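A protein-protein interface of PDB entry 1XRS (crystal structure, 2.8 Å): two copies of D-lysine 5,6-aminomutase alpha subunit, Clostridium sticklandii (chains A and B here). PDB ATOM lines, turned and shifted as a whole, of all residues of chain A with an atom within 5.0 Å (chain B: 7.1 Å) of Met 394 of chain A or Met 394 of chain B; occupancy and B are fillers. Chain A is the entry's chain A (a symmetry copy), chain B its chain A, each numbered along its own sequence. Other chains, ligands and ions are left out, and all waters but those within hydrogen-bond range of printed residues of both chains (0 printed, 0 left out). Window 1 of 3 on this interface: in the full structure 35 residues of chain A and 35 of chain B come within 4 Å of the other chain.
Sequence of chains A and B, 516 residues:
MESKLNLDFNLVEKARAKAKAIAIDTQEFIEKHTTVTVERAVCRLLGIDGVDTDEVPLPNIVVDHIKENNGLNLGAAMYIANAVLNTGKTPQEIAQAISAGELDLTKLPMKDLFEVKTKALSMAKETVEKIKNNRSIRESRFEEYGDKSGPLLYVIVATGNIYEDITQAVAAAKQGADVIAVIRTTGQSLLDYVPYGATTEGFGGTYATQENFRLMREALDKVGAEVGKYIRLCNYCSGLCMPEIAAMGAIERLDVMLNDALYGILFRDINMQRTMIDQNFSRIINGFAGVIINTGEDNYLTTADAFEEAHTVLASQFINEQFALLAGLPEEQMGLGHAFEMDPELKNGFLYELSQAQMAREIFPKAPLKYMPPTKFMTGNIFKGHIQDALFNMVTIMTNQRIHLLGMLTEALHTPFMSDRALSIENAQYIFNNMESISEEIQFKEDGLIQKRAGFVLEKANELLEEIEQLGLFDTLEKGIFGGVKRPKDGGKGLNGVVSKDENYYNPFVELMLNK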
ATOM      1  N   PHE A 350      -8.627   9.163  23.656  1.00  0.00           N
ATOM      2  CA  PHE A 350      -8.355  10.243  24.602  1.00  0.00           C
ATOM      3  C   PHE A 350      -9.570  10.541  25.517  1.00  0.00           C
ATOM      4  O   PHE A 350      -9.406  10.944  26.678  1.00  0.00           O
ATOM      5  CB  PHE A 350      -7.930  11.507  23.832  1.00  0.00           C
ATOM      6  CG  PHE A 350      -7.835  12.736  24.680  1.00  0.00           C
ATOM      7  CD1 PHE A 350      -8.876  13.640  24.725  1.00  0.00           C
ATOM      8  CD2 PHE A 350      -6.699  12.978  25.466  1.00  0.00           C
ATOM      9  CE1 PHE A 350      -8.785  14.788  25.559  1.00  0.00           C
ATOM     10  CE2 PHE A 350      -6.594  14.114  26.297  1.00  0.00           C
ATOM     11  CZ  PHE A 350      -7.637  15.013  26.341  1.00  0.00           C
ATOM     12  N   ALA A 390       1.915  15.048  25.276  1.00  0.00           N
ATOM     13  CA  ALA A 390       1.134  16.259  25.450  1.00  0.00           C
ATOM     14  C   ALA A 390      -0.322  15.909  25.807  1.00  0.00           C
ATOM     15  O   ALA A 390      -0.918  16.539  26.697  1.00  0.00           O
ATOM     16  CB  ALA A 390       1.196  17.117  24.145  1.00  0.00           C
ATOM     17  N   LEU A 391      -0.889  14.904  25.136  1.00  0.00           N
ATOM     18  CA  LEU A 391      -2.271  14.543  25.436  1.00  0.00           C
ATOM     19  C   LEU A 391      -2.316  13.996  26.858  1.00  0.00           C
ATOM     20  O   LEU A 391      -3.330  14.138  27.553  1.00  0.00           O
ATOM     21  CB  LEU A 391      -2.842  13.538  24.410  1.00  0.00           C
ATOM     22  CG  LEU A 391      -2.763  13.953  22.921  1.00  0.00           C
ATOM     23  CD1 LEU A 391      -3.762  13.117  22.104  1.00  0.00           C
ATOM     24  CD2 LEU A 391      -3.033  15.453  22.741  1.00  0.00           C
ATOM     25  N   PHE A 392      -1.190  13.404  27.281  1.00  0.00           N
ATOM     26  CA  PHE A 392      -1.014  12.857  28.629  1.00  0.00           C
ATOM     27  C   PHE A 392      -0.965  14.056  29.604  1.00  0.00           C
ATOM     28  O   PHE A 392      -1.690  14.110  30.616  1.00  0.00           O
ATOM     29  CB  PHE A 392       0.262  12.019  28.659  1.00  0.00           C
ATOM     30  CG  PHE A 392       0.855  11.809  30.040  1.00  0.00           C
ATOM     31  CD1 PHE A 392       0.102  11.263  31.078  1.00  0.00           C
ATOM     32  CD2 PHE A 392       2.192  12.142  30.291  1.00  0.00           C
ATOM     33  CE1 PHE A 392       0.658  11.052  32.335  1.00  0.00           C
ATOM     34  CE2 PHE A 392       2.751  11.932  31.545  1.00  0.00           C
ATOM     35  CZ  PHE A 392       1.988  11.387  32.564  1.00  0.00           C
ATOM     36  N   ASN A 393      -0.133  15.030  29.287  1.00  0.00           N
ATOM     37  CA  ASN A 393      -0.065  16.214  30.121  1.00  0.00           C
ATOM     38  C   ASN A 393      -1.460  16.852  30.261  1.00  0.00           C
ATOM     39  O   ASN A 393      -1.843  17.318  31.344  1.00  0.00           O
ATOM     40  CB  ASN A 393       0.937  17.217  29.527  1.00  0.00           C
ATOM     41  CG  ASN A 393       2.394  16.691  29.558  1.00  0.00           C
ATOM     42  OD1 ASN A 393       3.288  17.276  28.927  1.00  0.00           O
ATOM     43  ND2 ASN A 393       2.631  15.590  30.302  1.00  0.00           N
ATOM     44  N   MET A 394      -2.239  16.845  29.183  1.00  0.00           N
ATOM     45  CA  MET A 394      -3.562  17.472  29.245  1.00  0.00           C
ATOM     46  C   MET A 394      -4.452  16.829  30.288  1.00  0.00           C
ATOM     47  O   MET A 394      -5.088  17.537  31.082  1.00  0.00           O
ATOM     48  CB  MET A 394      -4.273  17.447  27.881  1.00  0.00           C
ATOM     49  CG  MET A 394      -3.624  18.317  26.785  1.00  0.00           C
ATOM     50  SD  MET A 394      -4.550  18.174  25.229  1.00  0.00           S
ATOM     51  CE  MET A 394      -6.124  18.723  25.966  1.00  0.00           C
ATOM     52  N   VAL A 395      -4.508  15.501  30.282  1.00  0.00           N
ATOM     53  CA  VAL A 395      -5.316  14.773  31.268  1.00  0.00           C
ATOM     54  C   VAL A 395      -4.967  15.198  32.719  1.00  0.00           C
ATOM     55  O   VAL A 395      -5.847  15.412  33.546  1.00  0.00           O
ATOM     56  CB  VAL A 395      -5.119  13.241  31.130  1.00  0.00           C
ATOM     57  CG1 VAL A 395      -5.738  12.514  32.307  1.00  0.00           C
ATOM     58  CG2 VAL A 395      -5.712  12.756  29.843  1.00  0.00           C
ATOM     59  N   THR A 396      -3.687  15.329  33.029  1.00  0.00           N
ATOM     60  CA  THR A 396      -3.326  15.734  34.365  1.00  0.00           C
ATOM     61  C   THR A 396      -3.959  17.073  34.771  1.00  0.00           C
ATOM     62  O   THR A 396      -4.581  17.168  35.816  1.00  0.00           O
ATOM     63  CB  THR A 396      -1.794  15.741  34.504  1.00  0.00           C
ATOM     64  OG1 THR A 396      -1.372  14.391  34.679  1.00  0.00           O
ATOM     65  CG2 THR A 396      -1.337  16.567  35.691  1.00  0.00           C
ATOM     66  N   ILE A 397      -3.813  18.104  33.959  1.00  0.00           N
ATOM     67  CA  ILE A 397      -4.410  19.392  34.296  1.00  0.00           C
ATOM     68  C   ILE A 397      -5.955  19.364  34.207  1.00  0.00           C
ATOM     69  O   ILE A 397      -6.610  20.113  34.926  1.00  0.00           O
ATOM     70  CB  ILE A 397      -3.842  20.545  33.391  1.00  0.00           C
ATOM     71  CG1 ILE A 397      -4.118  21.893  34.038  1.00  0.00           C
ATOM     72  CG2 ILE A 397      -4.455  20.503  31.985  1.00  0.00           C
ATOM     73  CD1 ILE A 397      -3.186  22.216  35.169  1.00  0.00           C
ATOM     74  N   MET A 398      -6.541  18.511  33.358  1.00  0.00           N
ATOM     75  CA  MET A 398      -8.014  18.452  33.259  1.00  0.00           C
ATOM     76  C   MET A 398      -8.620  17.713  34.440  1.00  0.00           C
ATOM     77  O   MET A 398      -9.793  17.899  34.778  1.00  0.00           O
ATOM     78  CB  MET A 398      -8.504  17.710  31.990  1.00  0.00           C
ATOM     79  CG  MET A 398      -7.931  18.211  30.651  1.00  0.00           C
ATOM     80  SD  MET A 398      -8.775  17.657  29.114  1.00  0.00           S
ATOM     81  CE  MET A 398     -10.442  18.334  29.514  1.00  0.00           C
ATOM     82  N   THR A 399      -7.829  16.858  35.068  1.00  0.00           N
ATOM     83  CA  THR A 399      -8.342  16.059  36.155  1.00  0.00           C
ATOM     84  C   THR A 399      -7.651  16.246  37.498  1.00  0.00           C
ATOM     85  O   THR A 399      -7.889  15.492  38.402  1.00  0.00           O
ATOM     86  CB  THR A 399      -8.301  14.574  35.762  1.00  0.00           C
ATOM     87  OG1 THR A 399      -6.942  14.180  35.540  1.00  0.00           O
ATOM     88  CG2 THR A 399      -9.100  14.329  34.479  1.00  0.00           C
ATOM     89  N   ILE A 431       1.431  23.214  28.330  1.00  0.00           N
ATOM     90  CA  ILE A 431       0.090  22.734  28.627  1.00  0.00           C
ATOM     91  C   ILE A 431      -0.451  23.106  30.019  1.00  0.00           C
ATOM     92  O   ILE A 431      -1.594  23.569  30.120  1.00  0.00           O
ATOM     93  CB  ILE A 431      -0.027  21.212  28.486  1.00  0.00           C
ATOM     94  CG1 ILE A 431       0.357  20.781  27.059  1.00  0.00           C
ATOM     95  CG2 ILE A 431      -1.450  20.779  28.818  1.00  0.00           C
ATOM     96  CD1 ILE A 431      -0.268  21.572  26.027  1.00  0.00           C
ATOM     97  N   MET A 435      -3.655  25.779  29.738  1.00  0.00           N
ATOM     98  CA  MET A 435      -4.953  25.191  30.059  1.00  0.00           C
ATOM     99  C   MET A 435      -5.239  25.224  31.562  1.00  0.00           C
ATOM    100  O   MET A 435      -6.085  24.466  32.038  1.00  0.00           O
ATOM    101  CB  MET A 435      -5.004  23.720  29.567  1.00  0.00           C
ATOM    102  CG  MET A 435      -4.657  23.529  28.105  1.00  0.00           C
ATOM    103  SD  MET A 435      -5.094  21.929  27.403  1.00  0.00           S
ATOM    104  CE  MET A 435      -5.351  21.171  28.811  1.00  0.00           C
ATOM    105  N   PHE B 340      -5.578  30.531  15.381  1.00  0.00           N
ATOM    106  CA  PHE B 340      -5.032  30.175  16.689  1.00  0.00           C
ATOM    107  C   PHE B 340      -3.713  30.981  16.753  1.00  0.00           C
ATOM    108  O   PHE B 340      -2.639  30.417  16.517  1.00  0.00           O
ATOM    109  CB  PHE B 340      -4.715  28.678  16.684  1.00  0.00           C
ATOM    110  CG  PHE B 340      -4.266  28.125  18.016  1.00  0.00           C
ATOM    111  CD1 PHE B 340      -5.195  27.632  18.933  1.00  0.00           C
ATOM    112  CD2 PHE B 340      -2.905  28.030  18.328  1.00  0.00           C
ATOM    113  CE1 PHE B 340      -4.780  27.040  20.138  1.00  0.00           C
ATOM    114  CE2 PHE B 340      -2.488  27.439  19.535  1.00  0.00           C
ATOM    115  CZ  PHE B 340      -3.428  26.940  20.437  1.00  0.00           C
ATOM    116  N   PHE B 350      -5.258  28.801  25.872  1.00  0.00           N
ATOM    117  CA  PHE B 350      -5.977  27.776  25.118  1.00  0.00           C
ATOM    118  C   PHE B 350      -7.504  27.815  25.385  1.00  0.00           C
ATOM    119  O   PHE B 350      -8.309  27.491  24.501  1.00  0.00           O
ATOM    120  CB  PHE B 350      -5.400  26.388  25.456  1.00  0.00           C
ATOM    121  CG  PHE B 350      -6.198  25.246  24.911  1.00  0.00           C
ATOM    122  CD1 PHE B 350      -7.107  24.582  25.707  1.00  0.00           C
ATOM    123  CD2 PHE B 350      -6.055  24.846  23.575  1.00  0.00           C
ATOM    124  CE1 PHE B 350      -7.881  23.518  25.166  1.00  0.00           C
ATOM    125  CE2 PHE B 350      -6.814  23.791  23.025  1.00  0.00           C
ATOM    126  CZ  PHE B 350      -7.725  23.132  23.823  1.00  0.00           C
ATOM    127  N   LEU B 354     -10.257  28.409  22.274  1.00  0.00           N
ATOM    128  CA  LEU B 354     -11.344  27.464  22.125  1.00  0.00           C
ATOM    129  C   LEU B 354     -12.658  28.218  22.171  1.00  0.00           C
ATOM    130  O   LEU B 354     -13.570  27.980  21.360  1.00  0.00           O
ATOM    131  CB  LEU B 354     -11.301  26.476  23.281  1.00  0.00           C
ATOM    132  CG  LEU B 354     -12.242  25.287  23.124  1.00  0.00           C
ATOM    133  CD1 LEU B 354     -11.886  24.533  21.836  1.00  0.00           C
ATOM    134  CD2 LEU B 354     -12.143  24.401  24.358  1.00  0.00           C
ATOM    135  N   TYR B 371     -10.124  27.631   9.765  1.00  0.00           N
ATOM    136  CA  TYR B 371      -9.363  27.936  10.963  1.00  0.00           C
ATOM    137  C   TYR B 371      -7.880  27.819  10.602  1.00  0.00           C
ATOM    138  O   TYR B 371      -7.446  26.797  10.055  1.00  0.00           O
ATOM    139  CB  TYR B 371      -9.797  26.971  12.078  1.00  0.00           C
ATOM    140  CG  TYR B 371      -9.392  27.419  13.438  1.00  0.00           C
ATOM    141  CD1 TYR B 371      -9.590  28.727  13.826  1.00  0.00           C
ATOM    142  CD2 TYR B 371      -8.776  26.538  14.338  1.00  0.00           C
ATOM    143  CE1 TYR B 371      -9.186  29.155  15.059  1.00  0.00           C
ATOM    144  CE2 TYR B 371      -8.367  26.966  15.596  1.00  0.00           C
ATOM    145  CZ  TYR B 371      -8.577  28.275  15.940  1.00  0.00           C
ATOM    146  OH  TYR B 371      -8.210  28.747  17.172  1.00  0.00           O
ATOM    147  N   ILE B 387       3.761  20.787  19.140  1.00  0.00           N
ATOM    148  CA  ILE B 387       2.712  20.681  20.146  1.00  0.00           C
ATOM    149  C   ILE B 387       1.738  21.843  20.091  1.00  0.00           C
ATOM    150  O   ILE B 387       0.551  21.673  20.381  1.00  0.00           O
ATOM    151  CB  ILE B 387       3.267  20.481  21.625  1.00  0.00           C
ATOM    152  CG1 ILE B 387       2.918  21.679  22.492  1.00  0.00           C
ATOM    153  CG2 ILE B 387       4.743  20.222  21.637  1.00  0.00           C
ATOM    154  CD1 ILE B 387       1.522  21.600  23.067  1.00  0.00           C
ATOM    155  N   ASP B 389       0.857  23.104  17.428  1.00  0.00           N
ATOM    156  CA  ASP B 389       0.085  22.826  16.222  1.00  0.00           C
ATOM    157  C   ASP B 389      -0.970  21.812  16.690  1.00  0.00           C
ATOM    158  O   ASP B 389      -2.080  21.721  16.168  1.00  0.00           O
ATOM    159  CB  ASP B 389       0.985  22.199  15.149  1.00  0.00           C
ATOM    160  CG  ASP B 389       1.622  23.239  14.223  1.00  0.00           C
ATOM    161  OD1 ASP B 389       2.581  22.909  13.495  1.00  0.00           O
ATOM    162  OD2 ASP B 389       1.161  24.400  14.211  1.00  0.00           O
ATOM    163  N   ALA B 390      -0.610  21.048  17.705  1.00  0.00           N
ATOM    164  CA  ALA B 390      -1.503  20.042  18.253  1.00  0.00           C
ATOM    165  C   ALA B 390      -2.657  20.713  19.020  1.00  0.00           C
ATOM    166  O   ALA B 390      -3.821  20.299  18.889  1.00  0.00           O
ATOM    167  CB  ALA B 390      -0.701  19.079  19.185  1.00  0.00           C
ATOM    168  N   LEU B 391      -2.347  21.751  19.802  1.00  0.00           N
ATOM    169  CA  LEU B 391      -3.408  22.411  20.555  1.00  0.00           C
ATOM    170  C   LEU B 391      -4.346  23.079  19.556  1.00  0.00           C
ATOM    171  O   LEU B 391      -5.549  23.210  19.817  1.00  0.00           O
ATOM    172  CB  LEU B 391      -2.845  23.418  21.585  1.00  0.00           C
ATOM    173  CG  LEU B 391      -1.809  22.866  22.593  1.00  0.00           C
ATOM    174  CD1 LEU B 391      -1.716  23.813  23.799  1.00  0.00           C
ATOM    175  CD2 LEU B 391      -2.166  21.443  23.044  1.00  0.00           C
ATOM    176  N   PHE B 392      -3.780  23.464  18.404  1.00  0.00           N
ATOM    177  CA  PHE B 392      -4.517  24.080  17.298  1.00  0.00           C
ATOM    178  C   PHE B 392      -5.430  22.987  16.696  1.00  0.00           C
ATOM    179  O   PHE B 392      -6.651  23.172  16.522  1.00  0.00           O
ATOM    180  CB  PHE B 392      -3.519  24.637  16.288  1.00  0.00           C
ATOM    181  CG  PHE B 392      -4.072  24.843  14.890  1.00  0.00           C
ATOM    182  CD1 PHE B 392      -5.207  25.621  14.665  1.00  0.00           C
ATOM    183  CD2 PHE B 392      -3.431  24.266  13.786  1.00  0.00           C
ATOM    184  CE1 PHE B 392      -5.696  25.824  13.380  1.00  0.00           C
ATOM    185  CE2 PHE B 392      -3.916  24.468  12.500  1.00  0.00           C
ATOM    186  CZ  PHE B 392      -5.044  25.245  12.296  1.00  0.00           C
ATOM    187  N   ASN B 393      -4.849  21.839  16.404  1.00  0.00           N
ATOM    188  CA  ASN B 393      -5.644  20.745  15.883  1.00  0.00           C
ATOM    189  C   ASN B 393      -6.804  20.420  16.844  1.00  0.00           C
ATOM    190  O   ASN B 393      -7.932  20.141  16.412  1.00  0.00           O
ATOM    191  CB  ASN B 393      -4.757  19.509  15.663  1.00  0.00           C
ATOM    192  CG  ASN B 393      -3.702  19.727  14.549  1.00  0.00           C
ATOM    193  OD1 ASN B 393      -2.774  18.917  14.394  1.00  0.00           O
ATOM    194  ND2 ASN B 393      -3.853  20.817  13.768  1.00  0.00           N
ATOM    195  N   MET B 394      -6.548  20.492  18.147  1.00  0.00           N
ATOM    196  CA  MET B 394      -7.601  20.157  19.108  1.00  0.00           C
ATOM    197  C   MET B 394      -8.809  21.057  18.970  1.00  0.00           C
ATOM    198  O   MET B 394      -9.948  20.568  18.942  1.00  0.00           O
ATOM    199  CB  MET B 394      -7.089  20.206  20.560  1.00  0.00           C
ATOM    200  CG  MET B 394      -6.048  19.128  20.927  1.00  0.00           C
ATOM    201  SD  MET B 394      -5.519  19.321  22.654  1.00  0.00           S
ATOM    202  CE  MET B 394      -7.207  19.173  23.323  1.00  0.00           C
ATOM    203  N   VAL B 395      -8.570  22.363  18.898  1.00  0.00           N
ATOM    204  CA  VAL B 395      -9.667  23.326  18.733  1.00  0.00           C
ATOM    205  C   VAL B 395     -10.563  22.968  17.518  1.00  0.00           C
ATOM    206  O   VAL B 395     -11.786  23.013  17.597  1.00  0.00           O
ATOM    207  CB  VAL B 395      -9.124  24.767  18.552  1.00  0.00           C
ATOM    208  CG1 VAL B 395     -10.232  25.706  18.119  1.00  0.00           C
ATOM    209  CG2 VAL B 395      -8.495  25.247  19.824  1.00  0.00           C
ATOM    210  N   THR B 396      -9.961  22.606  16.396  1.00  0.00           N
ATOM    211  CA  THR B 396     -10.762  22.255  15.250  1.00  0.00           C
ATOM    212  C   THR B 396     -11.750  21.115  15.542  1.00  0.00           C
ATOM    213  O   THR B 396     -12.933  21.242  15.276  1.00  0.00           O
ATOM    214  CB  THR B 396      -9.845  21.946  14.056  1.00  0.00           C
ATOM    215  OG1 THR B 396      -9.413  23.192  13.512  1.00  0.00           O
ATOM    216  CG2 THR B 396     -10.561  21.152  12.981  1.00  0.00           C
ATOM    217  N   ILE B 397     -11.281  20.009  16.090  1.00  0.00           N
ATOM    218  CA  ILE B 397     -12.183  18.905  16.399  1.00  0.00           C
ATOM    219  C   ILE B 397     -13.143  19.241  17.567  1.00  0.00           C
ATOM    220  O   ILE B 397     -14.248  18.708  17.607  1.00  0.00           O
ATOM    221  CB  ILE B 397     -11.392  17.584  16.718  1.00  0.00           C
ATOM    222  CG1 ILE B 397     -12.316  16.384  16.588  1.00  0.00           C
ATOM    223  CG2 ILE B 397     -10.782  17.627  18.125  1.00  0.00           C
ATOM    224  CD1 ILE B 397     -12.574  15.978  15.167  1.00  0.00           C
ATOM    225  N   MET B 398     -12.748  20.118  18.498  1.00  0.00           N
ATOM    226  CA  MET B 398     -13.645  20.467  19.620  1.00  0.00           C
ATOM    227  C   MET B 398     -14.745  21.416  19.174  1.00  0.00           C
ATOM    228  O   MET B 398     -15.805  21.505  19.799  1.00  0.00           O
ATOM    229  CB  MET B 398     -12.908  21.179  20.781  1.00  0.00           C
ATOM    230  CG  MET B 398     -11.668  20.455  21.339  1.00  0.00           C
ATOM    231  SD  MET B 398     -11.014  21.032  22.958  1.00  0.00           S
ATOM    232  CE  MET B 398     -12.549  20.749  23.938  1.00  0.00           C
ATOM    233  N   THR B 399     -14.494  22.143  18.096  1.00  0.00           N
ATOM    234  CA  THR B 399     -15.452  23.123  17.643  1.00  0.00           C
ATOM    235  C   THR B 399     -15.994  22.918  16.237  1.00  0.00           C
ATOM    236  O   THR B 399     -16.647  23.781  15.717  1.00  0.00           O
ATOM    237  CB  THR B 399     -14.839  24.528  17.754  1.00  0.00           C
ATOM    238  OG1 THR B 399     -13.694  24.614  16.897  1.00  0.00           O
ATOM    239  CG2 THR B 399     -14.399  24.816  19.193  1.00  0.00           C
ATOM    240  N   ASN B 400     -15.709  21.785  15.611  1.00  0.00           N
ATOM    241  CA  ASN B 400     -16.224  21.487  14.265  1.00  0.00           C
ATOM    242  C   ASN B 400     -15.928  22.485  13.138  1.00  0.00           C
ATOM    243  O   ASN B 400     -16.837  22.875  12.397  1.00  0.00           O
ATOM    244  CB  ASN B 400     -17.736  21.293  14.296  1.00  0.00           C
ATOM    245  CG  ASN B 400     -18.178  20.138  15.189  1.00  0.00           C
ATOM    246  OD1 ASN B 400     -17.673  19.009  15.087  1.00  0.00           O
ATOM    247  ND2 ASN B 400     -19.160  20.416  16.056  1.00  0.00           N
ATOM    248  N   HIS B 404      -9.461  23.067   7.461  1.00  0.00           N
ATOM    249  CA  HIS B 404      -8.308  23.074   8.351  1.00  0.00           C
ATOM    250  C   HIS B 404      -6.997  23.286   7.645  1.00  0.00           C
ATOM    251  O   HIS B 404      -6.500  22.400   6.969  1.00  0.00           O
ATOM    252  CB  HIS B 404      -8.268  21.758   9.149  1.00  0.00           C
ATOM    253  CG  HIS B 404      -7.294  21.757  10.291  1.00  0.00           C
ATOM    254  ND1 HIS B 404      -7.511  22.458  11.456  1.00  0.00           N
ATOM    255  CD2 HIS B 404      -6.133  21.083  10.471  1.00  0.00           C
ATOM    256  CE1 HIS B 404      -6.532  22.210  12.308  1.00  0.00           C
ATOM    257  NE2 HIS B 404      -5.682  21.378  11.733  1.00  0.00           N
ATOM    258  N   ASN B 427      -0.097  14.228  12.954  1.00  0.00           N
ATOM    259  CA  ASN B 427      -0.423  14.938  14.183  1.00  0.00           C
ATOM    260  C   ASN B 427      -1.924  15.245  14.147  1.00  0.00           C
ATOM    261  O   ASN B 427      -2.660  14.979  15.105  1.00  0.00           O
ATOM    262  CB  ASN B 427       0.392  16.237  14.277  1.00  0.00           C
ATOM    263  CG  ASN B 427       0.055  17.063  15.531  1.00  0.00           C
ATOM    264  OD1 ASN B 427      -1.025  16.906  16.102  1.00  0.00           O
ATOM    265  ND2 ASN B 427       0.968  17.968  15.942  1.00  0.00           N
ATOM    266  N   ILE B 431      -4.797  13.456  16.663  1.00  0.00           N
ATOM    267  CA  ILE B 431      -5.804  14.225  17.379  1.00  0.00           C
ATOM    268  C   ILE B 431      -7.239  14.096  16.839  1.00  0.00           C
ATOM    269  O   ILE B 431      -8.167  13.888  17.631  1.00  0.00           O
ATOM    270  CB  ILE B 431      -5.469  15.719  17.427  1.00  0.00           C
ATOM    271  CG1 ILE B 431      -4.101  15.936  18.098  1.00  0.00           C
ATOM    272  CG2 ILE B 431      -6.566  16.464  18.179  1.00  0.00           C
ATOM    273  CD1 ILE B 431      -3.939  15.201  19.329  1.00  0.00           C
ATOM    274  N   PHE B 432      -7.452  14.212  15.527  1.00  0.00           N
ATOM    275  CA  PHE B 432      -8.827  14.107  15.050  1.00  0.00           C
ATOM    276  C   PHE B 432      -9.459  12.791  15.372  1.00  0.00           C
ATOM    277  O   PHE B 432     -10.635  12.746  15.686  1.00  0.00           O
ATOM    278  CB  PHE B 432      -8.933  14.333  13.556  1.00  0.00           C
ATOM    279  CG  PHE B 432      -8.572  15.718  13.141  1.00  0.00           C
ATOM    280  CD1 PHE B 432      -8.384  16.030  11.798  1.00  0.00           C
ATOM    281  CD2 PHE B 432      -8.383  16.723  14.110  1.00  0.00           C
ATOM    282  CE1 PHE B 432      -8.009  17.315  11.431  1.00  0.00           C
ATOM    283  CE2 PHE B 432      -8.004  18.006  13.736  1.00  0.00           C
ATOM    284  CZ  PHE B 432      -7.816  18.302  12.401  1.00  0.00           C
ATOM    285  N   MET B 435      -9.717  12.122  19.569  1.00  0.00           N
ATOM    286  CA  MET B 435     -10.691  12.989  20.227  1.00  0.00           C
ATOM    287  C   MET B 435     -11.967  13.148  19.397  1.00  0.00           C
ATOM    288  O   MET B 435     -12.717  14.103  19.609  1.00  0.00           O
ATOM    289  CB  MET B 435     -10.070  14.390  20.473  1.00  0.00           C
ATOM    290  CG  MET B 435      -8.751  14.376  21.217  1.00  0.00           C
ATOM    291  SD  MET B 435      -8.211  15.964  21.874  1.00  0.00           S
ATOM    292  CE  MET B 435      -9.236  16.879  21.020  1.00  0.00           C
ATOM    293  N   ILE B 438     -15.104  14.388  21.011  1.00  0.00           N
ATOM    294  CA  ILE B 438     -14.915  15.389  22.046  1.00  0.00           C
ATOM    295  C   ILE B 438     -15.821  16.624  22.042  1.00  0.00           C
ATOM    296  O   ILE B 438     -16.020  17.220  23.079  1.00  0.00           O
ATOM    297  CB  ILE B 438     -13.428  15.849  22.131  1.00  0.00           C
ATOM    298  CG1 ILE B 438     -13.204  16.520  23.486  1.00  0.00           C
ATOM    299  CG2 ILE B 438     -13.046  16.798  20.977  1.00  0.00           C
ATOM    300  CD1 ILE B 438     -11.713  16.689  23.856  1.00  0.00           C
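The side-chain sulfur (SD) of Met 394 of chain A sits close to the side-chain sulfur (SD) of Met 394 of chain B (3.0 Å).
Among the printed residues, merely in contact across the chains: Phe 350 of chain A with Met 435 of chain B, Phe 350 of chain A with Ile 438 of chain B, Leu 391 of chain A with Ile 431 of chain B, Ile 431 of chain A with Ile 387 of chain B, Ile 431 of chain A with Leu 391 of chain B and Met 435 of chain A with Phe 350 of chain B.
Of chain B, only Met 394 comes within 4 Å of Met 394 of chain A. Of chain A, only Met 394 (2.9 Å) comes within 4 Å of Met 394 of chain B. Printed residues of chain B within 4 Å of Ile 431 of chain A: Ile 387 (3.5 Å) and Leu 391 (3.5 Å). Of the printed residues of chain A, Ile 431 of chain B touches Leu 391. Of the printed residues of chain A, Phe 350 of chain B touches Met 435 (3.6 Å). Val 395 of chain A touches none of the printed residues of chain B. The nearest residue of chain B that does not touch Met 394 of chain A is Leu 391 of chain B (4.6 Å). The nearest residue of chain A that does not touch Met 394 of chain B is Leu 391 of chain A (4.6 Å).
Hydrophobic or aromatic side chains of chain B within 4 Å of the printed part of chain A: Phe 350, Ile 387, Leu 391, Met 394, Ile 431, Met 435 and Ile 438. Hydrophobic or aromatic side chains of chain A within 4 Å of the printed part of chain B: Phe 350, Leu 391, Met 394, Ile 431 and Met 435. Among the printed residues, 7 pairs touch across the chains.
Phe 350 of chain A touches Met 435 of chain B, and with the chains exchanged Met 435 of chain A touches Phe 350 of chain B. Leu 391 of chain A touches Ile 431 of chain B, and with the chains exchanged Ile 431 of chain A touches Leu 391 of chain B. Met 394 of chain A touches its own counterpart, Met 394 of chain B.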
